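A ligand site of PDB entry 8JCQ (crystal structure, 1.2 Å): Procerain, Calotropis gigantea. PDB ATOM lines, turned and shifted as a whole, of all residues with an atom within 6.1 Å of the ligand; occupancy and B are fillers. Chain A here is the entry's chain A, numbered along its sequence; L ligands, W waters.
The backbone NH (N) of Cys 27 is in hydrogen-bond range of an oxygen (O1) of the ligand, at 2.8 Å. SG of Cys 27 is covalently linked to C2 of the ligand, at 1.8 Å. The side-chain amide nitrogen (NE2) of Gln 21 lies within hydrogen-bond range of an oxygen (O1) of the ligand, 2.8 Å away. The backbone NH (N) of Gly 68 lies within hydrogen-bond range of an oxygen (O4) of the ligand (3.0 Å). N2 of the ligand sits close to O of Gly 68, 3.5 Å away. N of Ser 26 sits at hydrogen-bond distance from O1 of the ligand (3.2 Å). An oxygen (O2) of the ligand sits at hydrogen-bond distance from a ring nitrogen (ND1) of His 157, at 3.3 Å.
The side-chain sulfur of Cys 27 lies close to a ring nitrogen (ND1) of His 157, 3.7 Å away. The side-chain sulfur of Cys 27 is in hydrogen-bond range of the backbone NH of Gly 158, 3.3 Å away. O of Gly 25 sits at hydrogen-bond distance from N of Gly 67. O of Cys 65 lies within hydrogen-bond range of N of Gly 25, at 2.9 Å. The side-chain hydroxyl of Ser 26 is in hydrogen-bond range of the side-chain sulfur of Cys 24. The side-chain hydroxyl of Ser 132 lies within hydrogen-bond range of the side-chain amide nitrogen of Gln 70 (3.2 Å). The backbone NH (N) of Asn 156 lies within hydrogen-bond range of the backbone carbonyl oxygen (O) of Ile 133, at 2.9 Å. The side-chain sulfur (SG) of Cys 24 is disulfide-bonded to the side-chain sulfur (SG) of Cys 65 (2.0 Å).
Merely in contact with the ligand: Cys 24 (3.9 Å), Gly 25 (3.1 Å), Trp 28 (3.1 Å), Gly 67 (3.3 Å), Gln 70 (3.7 Å), Ser 132 (3.3 Å), Ile 155 (3.8 Å), Asn 156 (3.5 Å) and Gly 158 (3.7 Å). 14 residues have an atom within 4 Å of the ligand: Gln 21, Cys 24, Gly 25, Ser 26, Cys 27, Trp 28, Gly 67, Gly 68, Gln 70, Ser 132, Ile 155, Asn 156, His 157 and Gly 158. The nearest printed residue that does not touch the ligand is Arg 69 (4.1 Å).
Water W3 lies within hydrogen-bond range of an oxygen (O5) of the ligand (2.6 Å) and the backbone carbonyl oxygen of Asn 156 (3.2 Å). Water W2 bridges the backbone carbonyl oxygen of Asn 156 (2.6 Å) and an oxygen (O2) of the ligand (2.7 Å). Water W4 lies within hydrogen-bond range of an oxygen (O2) of the ligand (2.8 Å), the indole nitrogen (NE1) of Trp 179 (2.9 Å) and the side-chain amide nitrogen (NE2) of Gln 21 (3.3 Å).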
ATOM      1  N   GLN A  21      -6.934  -2.421   5.337  1.00  0.00           N
ATOM      2  CA  GLN A  21      -7.526  -1.117   5.062  1.00  0.00           C
ATOM      3  C   GLN A  21      -6.508  -0.076   4.587  1.00  0.00           C
ATOM      4  O   GLN A  21      -6.901   0.990   4.099  1.00  0.00           O
ATOM      5  CB  GLN A  21      -8.212  -0.588   6.329  1.00  0.00           C
ATOM      6  CG  GLN A  21      -7.224  -0.279   7.472  1.00  0.00           C
ATOM      7  CD  GLN A  21      -7.937   0.299   8.655  1.00  0.00           C
ATOM      8  OE1 GLN A  21      -8.410  -0.457   9.512  1.00  0.00           O
ATOM      9  NE2 GLN A  21      -8.053   1.598   8.761  1.00  0.00           N
ATOM     10  N   CYS A  24      -6.167   4.482   4.917  1.00  0.00           N
ATOM     11  CA  CYS A  24      -7.470   5.115   4.991  1.00  0.00           C
ATOM     12  C   CYS A  24      -8.132   4.796   6.323  1.00  0.00           C
ATOM     13  O   CYS A  24      -8.061   3.661   6.801  1.00  0.00           O
ATOM     14  CB  CYS A  24      -8.274   4.516   3.828  1.00  0.00           C
ATOM     15  SG  CYS A  24     -10.018   4.868   3.683  1.00  0.00           S
ATOM     16  N   GLY A  25      -8.773   5.799   6.921  1.00  0.00           N
ATOM     17  CA  GLY A  25      -9.465   5.595   8.201  1.00  0.00           C
ATOM     18  C   GLY A  25     -10.846   4.995   8.020  1.00  0.00           C
ATOM     19  O   GLY A  25     -11.884   5.640   8.277  1.00  0.00           O
ATOM     20  N   SER A  26     -10.874   3.793   7.482  1.00  0.00           N
ATOM     21  CA  SER A  26     -12.125   3.127   7.118  1.00  0.00           C
ATOM     22  C   SER A  26     -12.428   1.940   8.031  1.00  0.00           C
ATOM     23  O   SER A  26     -13.201   1.050   7.665  1.00  0.00           O
ATOM     24  CB  SER A  26     -12.042   2.660   5.663  1.00  0.00           C
ATOM     25  OG  SER A  26     -10.852   1.914   5.527  1.00  0.00           O
ATOM     26  N   CYS A  27     -11.810   1.906   9.218  1.00  0.00           N
ATOM     27  CA  CYS A  27     -12.063   0.789  10.117  1.00  0.00           C
ATOM     28  C   CYS A  27     -13.557   0.562  10.377  1.00  0.00           C
ATOM     29  O   CYS A  27     -13.988  -0.574  10.565  1.00  0.00           O
ATOM     30  CB  CYS A  27     -11.315   0.966  11.450  1.00  0.00           C
ATOM     31  SG  CYS A  27     -11.861   2.291  12.461  1.00  0.00           S
ATOM     32  N   TRP A  28     -14.314   1.620  10.477  1.00  0.00           N
ATOM     33  CA  TRP A  28     -15.762   1.502  10.692  1.00  0.00           C
ATOM     34  C   TRP A  28     -16.401   0.619   9.630  1.00  0.00           C
ATOM     35  O   TRP A  28     -17.267  -0.205   9.943  1.00  0.00           O
ATOM     36  CB  TRP A  28     -16.393   2.894  10.666  1.00  0.00           C
ATOM     37  CG  TRP A  28     -16.158   3.659   9.360  1.00  0.00           C
ATOM     38  CD1 TRP A  28     -15.059   4.414   9.051  1.00  0.00           C
ATOM     39  CD2 TRP A  28     -17.087   3.807   8.272  1.00  0.00           C
ATOM     40  NE1 TRP A  28     -15.212   4.956   7.806  1.00  0.00           N
ATOM     41  CE2 TRP A  28     -16.446   4.598   7.291  1.00  0.00           C
ATOM     42  CE3 TRP A  28     -18.351   3.254   7.995  1.00  0.00           C
ATOM     43  CZ2 TRP A  28     -17.049   4.899   6.064  1.00  0.00           C
ATOM     44  CZ3 TRP A  28     -18.954   3.556   6.767  1.00  0.00           C
ATOM     45  CH2 TRP A  28     -18.297   4.388   5.828  1.00  0.00           C
ATOM     46  N   ALA A  29     -15.994   0.785   8.376  1.00  0.00           N
ATOM     47  CA  ALA A  29     -16.523  -0.013   7.284  1.00  0.00           C
ATOM     48  C   ALA A  29     -16.047  -1.452   7.350  1.00  0.00           C
ATOM     49  O   ALA A  29     -16.835  -2.382   7.130  1.00  0.00           O
ATOM     50  CB  ALA A  29     -16.122   0.659   5.945  1.00  0.00           C
ATOM     51  N   TYR A  63     -17.657   9.382   7.054  1.00  0.00           N
ATOM     52  CA  TYR A  63     -16.715  10.379   6.536  1.00  0.00           C
ATOM     53  C   TYR A  63     -15.620   9.708   5.717  1.00  0.00           C
ATOM     54  O   TYR A  63     -14.515  10.241   5.610  1.00  0.00           O
ATOM     55  CB  TYR A  63     -16.155  11.265   7.657  1.00  0.00           C
ATOM     56  CG  TYR A  63     -17.257  11.669   8.593  1.00  0.00           C
ATOM     57  CD1 TYR A  63     -18.178  12.652   8.250  1.00  0.00           C
ATOM     58  CD2 TYR A  63     -17.452  10.989   9.774  1.00  0.00           C
ATOM     59  CE1 TYR A  63     -19.249  12.973   9.121  1.00  0.00           C
ATOM     60  CE2 TYR A  63     -18.493  11.295  10.641  1.00  0.00           C
ATOM     61  CZ  TYR A  63     -19.391  12.282  10.305  1.00  0.00           C
ATOM     62  OH  TYR A  63     -20.420  12.551  11.182  1.00  0.00           O
ATOM     63  N   CYS A  65     -12.551   8.026   4.353  1.00  0.00           N
ATOM     64  CA  CYS A  65     -11.265   7.723   4.973  1.00  0.00           C
ATOM     65  C   CYS A  65     -10.977   8.584   6.194  1.00  0.00           C
ATOM     66  O   CYS A  65      -9.891   8.473   6.751  1.00  0.00           O
ATOM     67  CB  CYS A  65     -10.104   7.863   3.956  1.00  0.00           C
ATOM     68  SG  CYS A  65     -10.192   6.596   2.645  1.00  0.00           S
ATOM     69  N   LYS A  66     -11.943   9.414   6.593  1.00  0.00           N
ATOM     70  CA  LYS A  66     -11.872  10.287   7.752  1.00  0.00           C
ATOM     71  C   LYS A  66     -12.673   9.760   8.936  1.00  0.00           C
ATOM     72  O   LYS A  66     -12.974  10.514   9.871  1.00  0.00           O
ATOM     73  CB  LYS A  66     -12.288  11.735   7.379  1.00  0.00           C
ATOM     74  CG  LYS A  66     -11.504  12.415   6.250  1.00  0.00           C
ATOM     75  CD  LYS A  66     -12.128  13.795   5.750  1.00  0.00           C
ATOM     76  CE  LYS A  66     -13.621  13.652   5.360  1.00  0.00           C
ATOM     77  NZ  LYS A  66     -13.897  12.701   4.211  1.00  0.00           N
ATOM     78  N   GLY A  67     -13.019   8.461   8.940  1.00  0.00           N
ATOM     79  CA  GLY A  67     -13.708   7.875  10.062  1.00  0.00           C
ATOM     80  C   GLY A  67     -15.188   7.733   9.795  1.00  0.00           C
ATOM     81  O   GLY A  67     -15.725   8.227   8.795  1.00  0.00           O
ATOM     82  N   GLY A  68     -15.859   7.039  10.697  1.00  0.00           N
ATOM     83  CA  GLY A  68     -17.263   6.750  10.479  1.00  0.00           C
ATOM     84  C   GLY A  68     -17.796   5.872  11.589  1.00  0.00           C
ATOM     85  O   GLY A  68     -17.163   5.720  12.647  1.00  0.00           O
ATOM     86  N   ARG A  69     -18.976   5.302  11.347  1.00  0.00           N
ATOM     87  CA  ARG A  69     -19.697   4.513  12.357  1.00  0.00           C
ATOM     88  C   ARG A  69     -20.151   3.203  11.721  1.00  0.00           C
ATOM     89  O   ARG A  69     -20.795   3.185  10.663  1.00  0.00           O
ATOM     90  CB  ARG A  69     -20.956   5.248  12.819  1.00  0.00           C
ATOM     91  CG  ARG A  69     -20.683   6.637  13.382  1.00  0.00           C
ATOM     92  CD  ARG A  69     -22.012   7.371  13.624  1.00  0.00           C
ATOM     93  NE  ARG A  69     -21.810   8.797  13.891  1.00  0.00           N
ATOM     94  CZ  ARG A  69     -21.480   9.700  12.980  1.00  0.00           C
ATOM     95  NH1 ARG A  69     -21.373   9.398  11.702  1.00  0.00           N
ATOM     96  NH2 ARG A  69     -21.250  10.959  13.362  1.00  0.00           N
ATOM     97  N   GLN A  70     -19.847   2.072  12.397  1.00  0.00           N
ATOM     98  CA  GLN A  70     -20.359   0.791  11.925  1.00  0.00           C
ATOM     99  C   GLN A  70     -21.863   0.845  11.696  1.00  0.00           C
ATOM    100  O   GLN A  70     -22.369   0.303  10.717  1.00  0.00           O
ATOM    101  CB  GLN A  70     -20.051  -0.348  12.925  1.00  0.00           C
ATOM    102  CG  GLN A  70     -18.548  -0.656  13.114  1.00  0.00           C
ATOM    103  CD  GLN A  70     -17.954   0.049  14.287  1.00  0.00           C
ATOM    104  OE1 GLN A  70     -18.256   1.189  14.558  1.00  0.00           O
ATOM    105  NE2 GLN A  70     -17.080  -0.651  15.025  1.00  0.00           N
ATOM    106  N   ILE A 131     -17.117  -4.446  17.223  1.00  0.00           N
ATOM    107  CA  ILE A 131     -16.772  -3.793  18.494  1.00  0.00           C
ATOM    108  C   ILE A 131     -15.861  -2.626  18.188  1.00  0.00           C
ATOM    109  O   ILE A 131     -15.284  -2.498  17.085  1.00  0.00           O
ATOM    110  CB  ILE A 131     -16.133  -4.741  19.512  1.00  0.00           C
ATOM    111  CG1 ILE A 131     -14.927  -5.401  18.909  1.00  0.00           C
ATOM    112  CG2 ILE A 131     -17.166  -5.790  19.985  1.00  0.00           C
ATOM    113  CD1 ILE A 131     -14.043  -5.966  19.922  1.00  0.00           C
ATOM    114  N   SER A 132     -15.728  -1.754  19.177  1.00  0.00           N
ATOM    115  CA  SER A 132     -14.896  -0.552  19.097  1.00  0.00           C
ATOM    116  C   SER A 132     -13.990  -0.508  20.305  1.00  0.00           C
ATOM    117  O   SER A 132     -14.450  -0.677  21.448  1.00  0.00           O
ATOM    118  CB  SER A 132     -15.771   0.678  19.078  1.00  0.00           C
ATOM    119  OG  SER A 132     -16.618   0.598  17.915  1.00  0.00           O
ATOM    120  N   ILE A 133     -12.691  -0.293  20.052  1.00  0.00           N
ATOM    121  CA  ILE A 133     -11.672  -0.427  21.072  1.00  0.00           C
ATOM    122  C   ILE A 133     -10.762   0.797  21.091  1.00  0.00           C
ATOM    123  O   ILE A 133     -10.807   1.667  20.202  1.00  0.00           O
ATOM    124  CB  ILE A 133     -10.852  -1.724  20.932  1.00  0.00           C
ATOM    125  CG1 ILE A 133     -10.212  -1.794  19.533  1.00  0.00           C
ATOM    126  CG2 ILE A 133     -11.713  -2.923  21.250  1.00  0.00           C
ATOM    127  CD1 ILE A 133      -9.115  -2.841  19.415  1.00  0.00           C
ATOM    128  N   ILE A 155     -11.732   5.682  22.381  1.00  0.00           N
ATOM    129  CA  ILE A 155     -12.231   4.680  21.448  1.00  0.00           C
ATOM    130  C   ILE A 155     -11.880   5.175  20.047  1.00  0.00           C
ATOM    131  O   ILE A 155     -12.143   6.335  19.706  1.00  0.00           O
ATOM    132  CB  ILE A 155     -13.739   4.503  21.621  1.00  0.00           C
ATOM    133  CG1 ILE A 155     -14.043   3.815  22.960  1.00  0.00           C
ATOM    134  CG2 ILE A 155     -14.271   3.664  20.454  1.00  0.00           C
ATOM    135  CD1 ILE A 155     -15.223   4.406  23.718  1.00  0.00           C
ATOM    136  N   ASN A 156     -11.129   4.396  19.317  1.00  0.00           N
ATOM    137  CA  ASN A 156     -10.626   4.917  18.043  1.00  0.00           C
ATOM    138  C   ASN A 156     -10.510   3.851  16.952  1.00  0.00           C
ATOM    139  O   ASN A 156     -10.138   4.216  15.828  1.00  0.00           O
ATOM    140  CB  ASN A 156      -9.262   5.613  18.239  1.00  0.00           C
ATOM    141  CG  ASN A 156      -8.195   4.662  18.765  1.00  0.00           C
ATOM    142  OD1 ASN A 156      -8.454   3.488  18.978  1.00  0.00           O
ATOM    143  ND2 ASN A 156      -6.976   5.177  18.955  1.00  0.00           N
ATOM    144  N   HIS A 157     -10.843   2.598  17.197  1.00  0.00           N
ATOM    145  CA  HIS A 157     -10.641   1.587  16.164  1.00  0.00           C
ATOM    146  C   HIS A 157     -11.760   0.559  16.205  1.00  0.00           C
ATOM    147  O   HIS A 157     -12.094   0.006  17.264  1.00  0.00           O
ATOM    148  CB  HIS A 157      -9.261   0.936  16.332  1.00  0.00           C
ATOM    149  CG  HIS A 157      -8.866   0.029  15.198  1.00  0.00           C
ATOM    150  ND1 HIS A 157      -8.973   0.433  13.873  1.00  0.00           N
ATOM    151  CD2 HIS A 157      -8.317  -1.205  15.178  1.00  0.00           C
ATOM    152  CE1 HIS A 157      -8.537  -0.546  13.101  1.00  0.00           C
ATOM    153  NE2 HIS A 157      -8.136  -1.555  13.862  1.00  0.00           N
ATOM    154  N   GLY A 158     -12.340   0.259  15.048  1.00  0.00           N
ATOM    155  CA  GLY A 158     -13.385  -0.744  14.919  1.00  0.00           C
ATOM    156  C   GLY A 158     -12.809  -2.064  14.430  1.00  0.00           C
ATOM    157  O   GLY A 158     -12.072  -2.106  13.435  1.00  0.00           O
ATOM    158  N   TRP A 179      -5.608  -5.026   9.279  1.00  0.00           N
ATOM    159  CA  TRP A 179      -4.245  -4.559   9.025  1.00  0.00           C
ATOM    160  C   TRP A 179      -3.414  -5.586   8.261  1.00  0.00           C
ATOM    161  O   TRP A 179      -2.182  -5.514   8.285  1.00  0.00           O
ATOM    162  CB  TRP A 179      -3.553  -4.134  10.324  1.00  0.00           C
ATOM    163  CG  TRP A 179      -4.168  -2.979  11.050  1.00  0.00           C
ATOM    164  CD1 TRP A 179      -5.090  -2.092  10.554  1.00  0.00           C
ATOM    165  CD2 TRP A 179      -3.877  -2.557  12.387  1.00  0.00           C
ATOM    166  NE1 TRP A 179      -5.412  -1.144  11.514  1.00  0.00           N
ATOM    167  CE2 TRP A 179      -4.681  -1.419  12.652  1.00  0.00           C
ATOM    168  CE3 TRP A 179      -3.028  -3.049  13.399  1.00  0.00           C
ATOM    169  CZ2 TRP A 179      -4.700  -0.782  13.906  1.00  0.00           C
ATOM    170  CZ3 TRP A 179      -3.004  -2.394  14.623  1.00  0.00           C
ATOM    171  CH2 TRP A 179      -3.844  -1.286  14.885  1.00  0.00           C
HETATM  172  C1  LIG L   1      -9.520   3.368  11.594  1.00  0.00           C
HETATM  173  O1  LIG L   1      -9.637   3.315  10.362  1.00  0.00           O
HETATM  174  O2  LIG L   1      -8.395   3.150  12.160  1.00  0.00           O
HETATM  175  C2  LIG L   1     -10.759   3.686  12.441  1.00  0.00           C
HETATM  176  C3  LIG L   1     -11.420   4.991  11.975  1.00  0.00           C
HETATM  177  O3  LIG L   1     -10.574   6.144  12.169  1.00  0.00           O
HETATM  178  C4  LIG L   1     -12.843   5.278  12.455  1.00  0.00           C
HETATM  179  O4  LIG L   1     -13.768   5.095  11.746  1.00  0.00           O
HETATM  180  N1  LIG L   1     -13.013   5.669  13.765  1.00  0.00           N
HETATM  181  C5  LIG L   1     -14.324   5.923  14.373  1.00  0.00           C
HETATM  182  C6  LIG L   1     -14.310   5.065  15.677  1.00  0.00           C
HETATM  183  C7  LIG L   1     -14.088   3.550  15.478  1.00  0.00           C
HETATM  184  C8  LIG L   1     -14.390   2.787  16.780  1.00  0.00           C
HETATM  185  C9  LIG L   1     -15.133   3.102  14.466  1.00  0.00           C
HETATM  186  C10 LIG L   1     -14.514   7.438  14.581  1.00  0.00           C
HETATM  187  O5  LIG L   1     -13.543   8.166  14.488  1.00  0.00           O
HETATM  188  N2  LIG L   1     -15.718   7.961  14.845  1.00  0.00           N
HETATM  189  C11 LIG L   1     -16.965   7.274  15.039  1.00  0.00           C
HETATM  190  O   HOH W   1      -6.785   5.419  10.553  1.00  0.00           O
HETATM  191  O   HOH W   2      -7.800   4.090  14.639  1.00  0.00           O
HETATM  192  O   HOH W   3     -11.376   7.194  15.618  1.00  0.00           O
HETATM  193  O   HOH W   4      -6.153   1.698  11.491  1.00  0.00           O
